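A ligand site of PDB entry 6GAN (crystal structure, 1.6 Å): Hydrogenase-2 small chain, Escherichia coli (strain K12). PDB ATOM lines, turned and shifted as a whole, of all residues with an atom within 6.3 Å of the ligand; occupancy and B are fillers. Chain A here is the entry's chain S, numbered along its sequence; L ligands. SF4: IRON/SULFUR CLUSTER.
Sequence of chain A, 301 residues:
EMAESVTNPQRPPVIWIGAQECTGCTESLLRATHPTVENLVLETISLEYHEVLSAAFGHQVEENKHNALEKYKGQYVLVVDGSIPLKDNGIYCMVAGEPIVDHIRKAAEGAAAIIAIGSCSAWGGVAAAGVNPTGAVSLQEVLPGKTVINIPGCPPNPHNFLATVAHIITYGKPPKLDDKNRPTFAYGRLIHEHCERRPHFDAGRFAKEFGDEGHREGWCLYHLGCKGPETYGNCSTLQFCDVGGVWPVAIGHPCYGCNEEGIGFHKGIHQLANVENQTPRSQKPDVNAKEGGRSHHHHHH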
ATOM      1  N   ILE A 191     -18.797   7.791   1.356  1.00  0.00           N
ATOM      2  CA  ILE A 191     -18.605   8.077   2.738  1.00  0.00           C
ATOM      3  C   ILE A 191     -17.101   8.133   3.105  1.00  0.00           C
ATOM      4  O   ILE A 191     -16.658   9.023   3.784  1.00  0.00           O
ATOM      5  CB  ILE A 191     -19.393   7.061   3.628  1.00  0.00           C
ATOM      6  CG1 ILE A 191     -20.903   7.330   3.490  1.00  0.00           C
ATOM      7  CG2 ILE A 191     -18.912   7.050   5.072  1.00  0.00           C
ATOM      8  CD1 ILE A 191     -21.779   6.220   4.070  1.00  0.00           C
ATOM      9  N   HIS A 192     -16.327   7.211   2.539  1.00  0.00           N
ATOM     10  CA  HIS A 192     -14.872   7.132   2.755  1.00  0.00           C
ATOM     11  C   HIS A 192     -14.127   8.296   2.160  1.00  0.00           C
ATOM     12  O   HIS A 192     -12.963   8.529   2.558  1.00  0.00           O
ATOM     13  CB  HIS A 192     -14.378   5.851   2.075  1.00  0.00           C
ATOM     14  CG  HIS A 192     -12.917   5.527   2.222  1.00  0.00           C
ATOM     15  ND1 HIS A 192     -12.365   5.059   3.403  1.00  0.00           N
ATOM     16  CD2 HIS A 192     -11.900   5.594   1.322  1.00  0.00           C
ATOM     17  CE1 HIS A 192     -11.068   4.805   3.199  1.00  0.00           C
ATOM     18  NE2 HIS A 192     -10.763   5.146   1.953  1.00  0.00           N
ATOM     19  N   GLU A 193     -14.734   9.009   1.202  1.00  0.00           N
ATOM     20  CA  GLU A 193     -14.081  10.191   0.616  1.00  0.00           C
ATOM     21  C   GLU A 193     -14.502  11.439   1.384  1.00  0.00           C
ATOM     22  O   GLU A 193     -14.182  12.562   0.979  1.00  0.00           O
ATOM     23  CB  GLU A 193     -14.337  10.340  -0.866  1.00  0.00           C
ATOM     24  CG  GLU A 193     -13.649   9.277  -1.721  1.00  0.00           C
ATOM     25  CD  GLU A 193     -12.135   9.219  -1.516  1.00  0.00           C
ATOM     26  OE1 GLU A 193     -11.581   8.161  -1.112  1.00  0.00           O
ATOM     27  OE2 GLU A 193     -11.515  10.272  -1.697  1.00  0.00           O
ATOM     28  N   CYS A 195     -14.733  10.982   5.358  1.00  0.00           N
ATOM     29  CA  CYS A 195     -14.807  10.363   6.702  1.00  0.00           C
ATOM     30  C   CYS A 195     -13.685  10.849   7.559  1.00  0.00           C
ATOM     31  O   CYS A 195     -12.483  10.799   7.110  1.00  0.00           O
ATOM     32  CB  CYS A 195     -14.642   8.862   6.534  1.00  0.00           C
ATOM     33  SG  CYS A 195     -14.684   7.939   8.097  1.00  0.00           S
ATOM     34  N   GLU A 196     -14.042  11.235   8.783  1.00  0.00           N
ATOM     35  CA  GLU A 196     -13.099  11.732   9.755  1.00  0.00           C
ATOM     36  C   GLU A 196     -12.078  10.694  10.225  1.00  0.00           C
ATOM     37  O   GLU A 196     -11.099  11.060  10.865  1.00  0.00           O
ATOM     38  CB  GLU A 196     -13.802  12.365  10.932  1.00  0.00           C
ATOM     39  CG  GLU A 196     -14.529  11.353  11.826  1.00  0.00           C
ATOM     40  CD  GLU A 196     -15.997  11.074  11.454  1.00  0.00           C
ATOM     41  OE1 GLU A 196     -16.450  11.317  10.281  1.00  0.00           O
ATOM     42  OE2 GLU A 196     -16.699  10.590  12.394  1.00  0.00           O
ATOM     43  N   ARG A 197     -12.260   9.407   9.867  1.00  0.00           N
ATOM     44  CA  ARG A 197     -11.275   8.400  10.283  1.00  0.00           C
ATOM     45  C   ARG A 197     -10.282   8.099   9.162  1.00  0.00           C
ATOM     46  O   ARG A 197      -9.394   7.248   9.329  1.00  0.00           O
ATOM     47  CB  ARG A 197     -11.936   7.132  10.793  1.00  0.00           C
ATOM     48  CG  ARG A 197     -12.791   7.485  12.028  1.00  0.00           C
ATOM     49  CD  ARG A 197     -13.251   6.293  12.792  1.00  0.00           C
ATOM     50  NE  ARG A 197     -14.016   6.711  13.971  1.00  0.00           N
ATOM     51  CZ  ARG A 197     -14.289   5.939  15.011  1.00  0.00           C
ATOM     52  NH1 ARG A 197     -13.859   4.686  15.056  1.00  0.00           N
ATOM     53  NH2 ARG A 197     -14.971   6.437  16.021  1.00  0.00           N
ATOM     54  N   ARG A 198     -10.388   8.845   8.068  1.00  0.00           N
ATOM     55  CA  ARG A 198      -9.456   8.605   6.947  1.00  0.00           C
ATOM     56  C   ARG A 198      -7.972   8.716   7.356  1.00  0.00           C
ATOM     57  O   ARG A 198      -7.146   7.964   6.827  1.00  0.00           O
ATOM     58  CB  ARG A 198      -9.789   9.540   5.773  1.00  0.00           C
ATOM     59  CG  ARG A 198      -8.933   9.355   4.543  1.00  0.00           C
ATOM     60  CD  ARG A 198      -8.947   7.936   3.938  1.00  0.00           C
ATOM     61  NE  ARG A 198      -8.154   7.992   2.721  1.00  0.00           N
ATOM     62  CZ  ARG A 198      -8.636   8.276   1.534  1.00  0.00           C
ATOM     63  NH1 ARG A 198      -9.940   8.426   1.342  1.00  0.00           N
ATOM     64  NH2 ARG A 198      -7.807   8.440   0.507  1.00  0.00           N
ATOM     65  N   PRO A 199      -7.639   9.668   8.229  1.00  0.00           N
ATOM     66  CA  PRO A 199      -6.214   9.721   8.638  1.00  0.00           C
ATOM     67  C   PRO A 199      -5.679   8.403   9.246  1.00  0.00           C
ATOM     68  O   PRO A 199      -4.478   8.040   9.086  1.00  0.00           O
ATOM     69  CB  PRO A 199      -6.222  10.816   9.695  1.00  0.00           C
ATOM     70  CG  PRO A 199      -7.393  11.684   9.351  1.00  0.00           C
ATOM     71  CD  PRO A 199      -8.431  10.747   8.837  1.00  0.00           C
ATOM     72  N   PHE A 201      -7.023   5.371   8.589  1.00  0.00           N
ATOM     73  CA  PHE A 201      -6.930   4.464   7.430  1.00  0.00           C
ATOM     74  C   PHE A 201      -5.562   4.679   6.770  1.00  0.00           C
ATOM     75  O   PHE A 201      -4.859   3.723   6.447  1.00  0.00           O
ATOM     76  CB  PHE A 201      -8.051   4.786   6.416  1.00  0.00           C
ATOM     77  CG  PHE A 201      -8.035   3.935   5.185  1.00  0.00           C
ATOM     78  CD1 PHE A 201      -7.376   4.369   4.057  1.00  0.00           C
ATOM     79  CD2 PHE A 201      -8.780   2.786   5.120  1.00  0.00           C
ATOM     80  CE1 PHE A 201      -7.362   3.615   2.900  1.00  0.00           C
ATOM     81  CE2 PHE A 201      -8.798   2.005   3.958  1.00  0.00           C
ATOM     82  CZ  PHE A 201      -8.067   2.404   2.843  1.00  0.00           C
ATOM     83  N   PHE A 206      -5.838   0.758  12.650  1.00  0.00           N
ATOM     84  CA  PHE A 206      -7.097   0.006  12.473  1.00  0.00           C
ATOM     85  C   PHE A 206      -7.522  -0.673  13.754  1.00  0.00           C
ATOM     86  O   PHE A 206      -6.729  -1.291  14.450  1.00  0.00           O
ATOM     87  CB  PHE A 206      -6.936  -1.078  11.413  1.00  0.00           C
ATOM     88  CG  PHE A 206      -6.623  -0.569  10.032  1.00  0.00           C
ATOM     89  CD1 PHE A 206      -7.534   0.190   9.309  1.00  0.00           C
ATOM     90  CD2 PHE A 206      -5.422  -0.927   9.404  1.00  0.00           C
ATOM     91  CE1 PHE A 206      -7.280   0.619   8.038  1.00  0.00           C
ATOM     92  CE2 PHE A 206      -5.146  -0.474   8.127  1.00  0.00           C
ATOM     93  CZ  PHE A 206      -6.090   0.289   7.431  1.00  0.00           C
ATOM     94  N   TRP A 219     -10.033   4.569  16.061  1.00  0.00           N
ATOM     95  CA  TRP A 219      -9.330   4.283  14.828  1.00  0.00           C
ATOM     96  C   TRP A 219     -10.259   3.835  13.707  1.00  0.00           C
ATOM     97  O   TRP A 219     -11.468   3.593  13.940  1.00  0.00           O
ATOM     98  CB  TRP A 219      -8.229   3.228  15.069  1.00  0.00           C
ATOM     99  CG  TRP A 219      -7.036   3.784  15.820  1.00  0.00           C
ATOM    100  CD1 TRP A 219      -6.886   5.053  16.316  1.00  0.00           C
ATOM    101  CD2 TRP A 219      -5.832   3.082  16.142  1.00  0.00           C
ATOM    102  NE1 TRP A 219      -5.652   5.176  16.929  1.00  0.00           N
ATOM    103  CE2 TRP A 219      -5.000   3.971  16.855  1.00  0.00           C
ATOM    104  CE3 TRP A 219      -5.379   1.778  15.923  1.00  0.00           C
ATOM    105  CZ2 TRP A 219      -3.727   3.594  17.340  1.00  0.00           C
ATOM    106  CZ3 TRP A 219      -4.122   1.409  16.419  1.00  0.00           C
ATOM    107  CH2 TRP A 219      -3.328   2.311  17.106  1.00  0.00           C
ATOM    108  N   CYS A 220      -9.711   3.716  12.489  1.00  0.00           N
ATOM    109  CA  CYS A 220     -10.550   3.352  11.336  1.00  0.00           C
ATOM    110  C   CYS A 220     -11.081   1.923  11.497  1.00  0.00           C
ATOM    111  O   CYS A 220     -10.430   1.038  12.106  1.00  0.00           O
ATOM    112  CB  CYS A 220      -9.736   3.484  10.034  1.00  0.00           C
ATOM    113  SG  CYS A 220     -10.324   2.735   8.531  1.00  0.00           S
ATOM    114  N   LEU A 221     -12.317   1.729  10.989  1.00  0.00           N
ATOM    115  CA  LEU A 221     -13.007   0.471  11.044  1.00  0.00           C
ATOM    116  C   LEU A 221     -12.978  -0.377   9.773  1.00  0.00           C
ATOM    117  O   LEU A 221     -13.748  -1.355   9.638  1.00  0.00           O
ATOM    118  CB  LEU A 221     -14.447   0.761  11.488  1.00  0.00           C
ATOM    119  CG  LEU A 221     -14.597   1.741  12.678  1.00  0.00           C
ATOM    120  CD1 LEU A 221     -16.091   1.908  13.067  1.00  0.00           C
ATOM    121  CD2 LEU A 221     -13.859   1.277  13.888  1.00  0.00           C
ATOM    122  N   TYR A 222     -12.088  -0.028   8.838  1.00  0.00           N
ATOM    123  CA  TYR A 222     -11.934  -0.787   7.598  1.00  0.00           C
ATOM    124  C   TYR A 222     -11.826  -2.286   7.851  1.00  0.00           C
ATOM    125  O   TYR A 222     -12.494  -3.081   7.181  1.00  0.00           O
ATOM    126  CB  TYR A 222     -10.717  -0.269   6.726  1.00  0.00           C
ATOM    127  CG  TYR A 222     -10.594  -1.055   5.445  1.00  0.00           C
ATOM    128  CD1 TYR A 222     -11.489  -0.865   4.411  1.00  0.00           C
ATOM    129  CD2 TYR A 222      -9.667  -2.067   5.322  1.00  0.00           C
ATOM    130  CE1 TYR A 222     -11.450  -1.618   3.269  1.00  0.00           C
ATOM    131  CE2 TYR A 222      -9.608  -2.863   4.183  1.00  0.00           C
ATOM    132  CZ  TYR A 222     -10.503  -2.618   3.146  1.00  0.00           C
ATOM    133  OH  TYR A 222     -10.475  -3.404   2.013  1.00  0.00           O
ATOM    134  N   HIS A 223     -10.972  -2.668   8.806  1.00  0.00           N
ATOM    135  CA  HIS A 223     -10.755  -4.108   9.016  1.00  0.00           C
ATOM    136  C   HIS A 223     -11.835  -4.757   9.840  1.00  0.00           C
ATOM    137  O   HIS A 223     -11.786  -5.961  10.051  1.00  0.00           O
ATOM    138  CB  HIS A 223      -9.345  -4.399   9.551  1.00  0.00           C
ATOM    139  CG  HIS A 223      -8.312  -4.402   8.465  1.00  0.00           C
ATOM    140  ND1 HIS A 223      -8.152  -5.471   7.613  1.00  0.00           N
ATOM    141  CD2 HIS A 223      -7.487  -3.429   8.030  1.00  0.00           C
ATOM    142  CE1 HIS A 223      -7.233  -5.155   6.707  1.00  0.00           C
ATOM    143  NE2 HIS A 223      -6.829  -3.917   6.923  1.00  0.00           N
ATOM    144  N   CYS A 226     -15.875  -2.085   7.332  1.00  0.00           N
ATOM    145  CA  CYS A 226     -16.502  -0.801   6.974  1.00  0.00           C
ATOM    146  C   CYS A 226     -16.728  -0.680   5.462  1.00  0.00           C
ATOM    147  O   CYS A 226     -15.819  -0.892   4.641  1.00  0.00           O
ATOM    148  CB  CYS A 226     -15.723   0.359   7.541  1.00  0.00           C
ATOM    149  SG  CYS A 226     -16.562   1.921   7.241  1.00  0.00           S
ATOM    150  N   LYS A 227     -17.966  -0.340   5.089  1.00  0.00           N
ATOM    151  CA  LYS A 227     -18.332  -0.237   3.695  1.00  0.00           C
ATOM    152  C   LYS A 227     -18.297   1.171   3.169  1.00  0.00           C
ATOM    153  O   LYS A 227     -18.693   1.460   2.002  1.00  0.00           O
ATOM    154  CB  LYS A 227     -19.717  -0.839   3.475  1.00  0.00           C
ATOM    155  CG  LYS A 227     -19.806  -2.312   3.883  1.00  0.00           C
ATOM    156  CD  LYS A 227     -18.690  -3.183   3.265  1.00  0.00           C
ATOM    157  CE  LYS A 227     -18.979  -4.654   3.417  1.00  0.00           C
ATOM    158  NZ  LYS A 227     -19.065  -5.071   4.854  1.00  0.00           N
ATOM    159  N   GLY A 228     -17.801   2.066   3.992  1.00  0.00           N
ATOM    160  CA  GLY A 228     -17.624   3.449   3.568  1.00  0.00           C
ATOM    161  C   GLY A 228     -16.952   3.601   2.223  1.00  0.00           C
ATOM    162  O   GLY A 228     -17.292   4.462   1.464  1.00  0.00           O
ATOM    163  N   PRO A 229     -15.954   2.762   1.919  1.00  0.00           N
ATOM    164  CA  PRO A 229     -15.284   2.945   0.605  1.00  0.00           C
ATOM    165  C   PRO A 229     -16.115   2.659  -0.651  1.00  0.00           C
ATOM    166  O   PRO A 229     -15.671   3.010  -1.771  1.00  0.00           O
ATOM    167  CB  PRO A 229     -14.122   1.958   0.692  1.00  0.00           C
ATOM    168  CG  PRO A 229     -13.813   1.841   2.149  1.00  0.00           C
ATOM    169  CD  PRO A 229     -15.182   1.914   2.852  1.00  0.00           C
ATOM    170  N   TRP A 247     -23.261   8.820  14.121  1.00  0.00           N
ATOM    171  CA  TRP A 247     -23.455   7.944  12.993  1.00  0.00           C
ATOM    172  C   TRP A 247     -22.804   6.618  13.341  1.00  0.00           C
ATOM    173  O   TRP A 247     -22.132   6.552  14.365  1.00  0.00           O
ATOM    174  CB  TRP A 247     -22.933   8.535  11.707  1.00  0.00           C
ATOM    175  CG  TRP A 247     -21.435   8.725  11.502  1.00  0.00           C
ATOM    176  CD1 TRP A 247     -20.611   9.599  12.159  1.00  0.00           C
ATOM    177  CD2 TRP A 247     -20.644   8.101  10.495  1.00  0.00           C
ATOM    178  NE1 TRP A 247     -19.343   9.566  11.620  1.00  0.00           N
ATOM    179  CE2 TRP A 247     -19.317   8.638  10.610  1.00  0.00           C
ATOM    180  CE3 TRP A 247     -20.920   7.186   9.487  1.00  0.00           C
ATOM    181  CZ2 TRP A 247     -18.301   8.257   9.766  1.00  0.00           C
ATOM    182  CZ3 TRP A 247     -19.890   6.773   8.667  1.00  0.00           C
ATOM    183  CH2 TRP A 247     -18.597   7.349   8.782  1.00  0.00           C
ATOM    184  N   VAL A 249     -20.212   4.744  12.418  1.00  0.00           N
ATOM    185  CA  VAL A 249     -18.744   4.704  12.602  1.00  0.00           C
ATOM    186  C   VAL A 249     -18.353   5.485  13.830  1.00  0.00           C
ATOM    187  O   VAL A 249     -17.556   5.025  14.635  1.00  0.00           O
ATOM    188  CB  VAL A 249     -18.027   5.199  11.341  1.00  0.00           C
ATOM    189  CG1 VAL A 249     -16.558   5.561  11.615  1.00  0.00           C
ATOM    190  CG2 VAL A 249     -18.163   4.171  10.221  1.00  0.00           C
ATOM    191  N   PRO A 254     -18.699  -0.409  12.032  1.00  0.00           N
ATOM    192  CA  PRO A 254     -18.496  -0.139  10.607  1.00  0.00           C
ATOM    193  C   PRO A 254     -19.757   0.231   9.864  1.00  0.00           C
ATOM    194  O   PRO A 254     -20.852  -0.218  10.222  1.00  0.00           O
ATOM    195  CB  PRO A 254     -17.966  -1.487  10.045  1.00  0.00           C
ATOM    196  CG  PRO A 254     -18.222  -2.500  11.102  1.00  0.00           C
ATOM    197  CD  PRO A 254     -18.223  -1.752  12.412  1.00  0.00           C
ATOM    198  N   CYS A 255     -19.637   1.064   8.847  1.00  0.00           N
ATOM    199  CA  CYS A 255     -20.733   1.182   7.834  1.00  0.00           C
ATOM    200  C   CYS A 255     -20.981  -0.217   7.209  1.00  0.00           C
ATOM    201  O   CYS A 255     -20.001  -0.953   6.952  1.00  0.00           O
ATOM    202  CB  CYS A 255     -20.376   2.210   6.772  1.00  0.00           C
ATOM    203  SG  CYS A 255     -21.488   2.336   5.323  1.00  0.00           S
HETATM  204 FE1  SF4 L   1     -12.151   3.854   7.731  1.00  0.00          FE
HETATM  205 FE2  SF4 L   1     -14.776   3.387   7.048  1.00  0.00          FE
HETATM  206 FE3  SF4 L   1     -13.099   4.639   5.289  1.00  0.00          FE
HETATM  207 FE4  SF4 L   1     -13.962   5.889   7.507  1.00  0.00          FE
HETATM  208  S1  SF4 L   1     -15.289   5.186   5.738  1.00  0.00           S
HETATM  209  S2  SF4 L   1     -11.770   5.866   6.763  1.00  0.00           S
HETATM  210  S3  SF4 L   1     -13.999   4.164   9.029  1.00  0.00           S
HETATM  211  S4  SF4 L   1     -12.917   2.508   5.988  1.00  0.00           S
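The guanidinium group (NH1) of Arg 198 is in salt-bridge range of the side-chain carboxylate (OE1) of Glu 193. N of His 192 lies within hydrogen-bond range of O of Gly 228 (3.1 Å). The backbone carbonyl oxygen (O) of Val 249 is in hydrogen-bond range of the guanidinium group (NH2) of Arg 197, 3.3 Å away. The backbone NH of Cys 226 lies within hydrogen-bond range of the backbone carbonyl oxygen of Leu 221 (3.2 Å). The guanidinium group (NH1) of Arg 198 lies within hydrogen-bond range of the backbone carbonyl oxygen (O) of His 192. N of Gly 228 lies close to SG of Cys 226 (3.5 Å). SG of Cys 226 lies close to N of Cys 255 (3.6 Å). The side-chain sulfur (SG) of Cys 220 sits close to the backbone NH (N) of Tyr 222 (3.3 Å).
A sulfur (S2) of the ligand lies close to the backbone carbonyl oxygen (O) of Arg 197 (3.8 Å). Merely in contact with the ligand: Phe 201, Tyr 222, Gly 228, Pro 229 and Val 249. Of the 23 residues printed, 12 come within 4 Å of the ligand. The nearest printed residue that does not touch the ligand is Ile 191 (4.1 Å).
The backbone NH (N) of Arg 198 sits close to a sulfur (S2) of the ligand. An iron atom (FE1) of the ligand is bound by the side-chain sulfur (SG) of Cys 220, 2.3 Å away. ND1 of His 192 is bound to FE3 of the ligand (2.1 Å). The backbone NH (N) of Leu 221 sits close to a sulfur (S3) of the ligand, 3.5 Å away. SG of Cys 195 is bound to FE4 of the ligand (2.3 Å). FE2 of the ligand is bound by SG of Cys 226 (2.3 Å).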
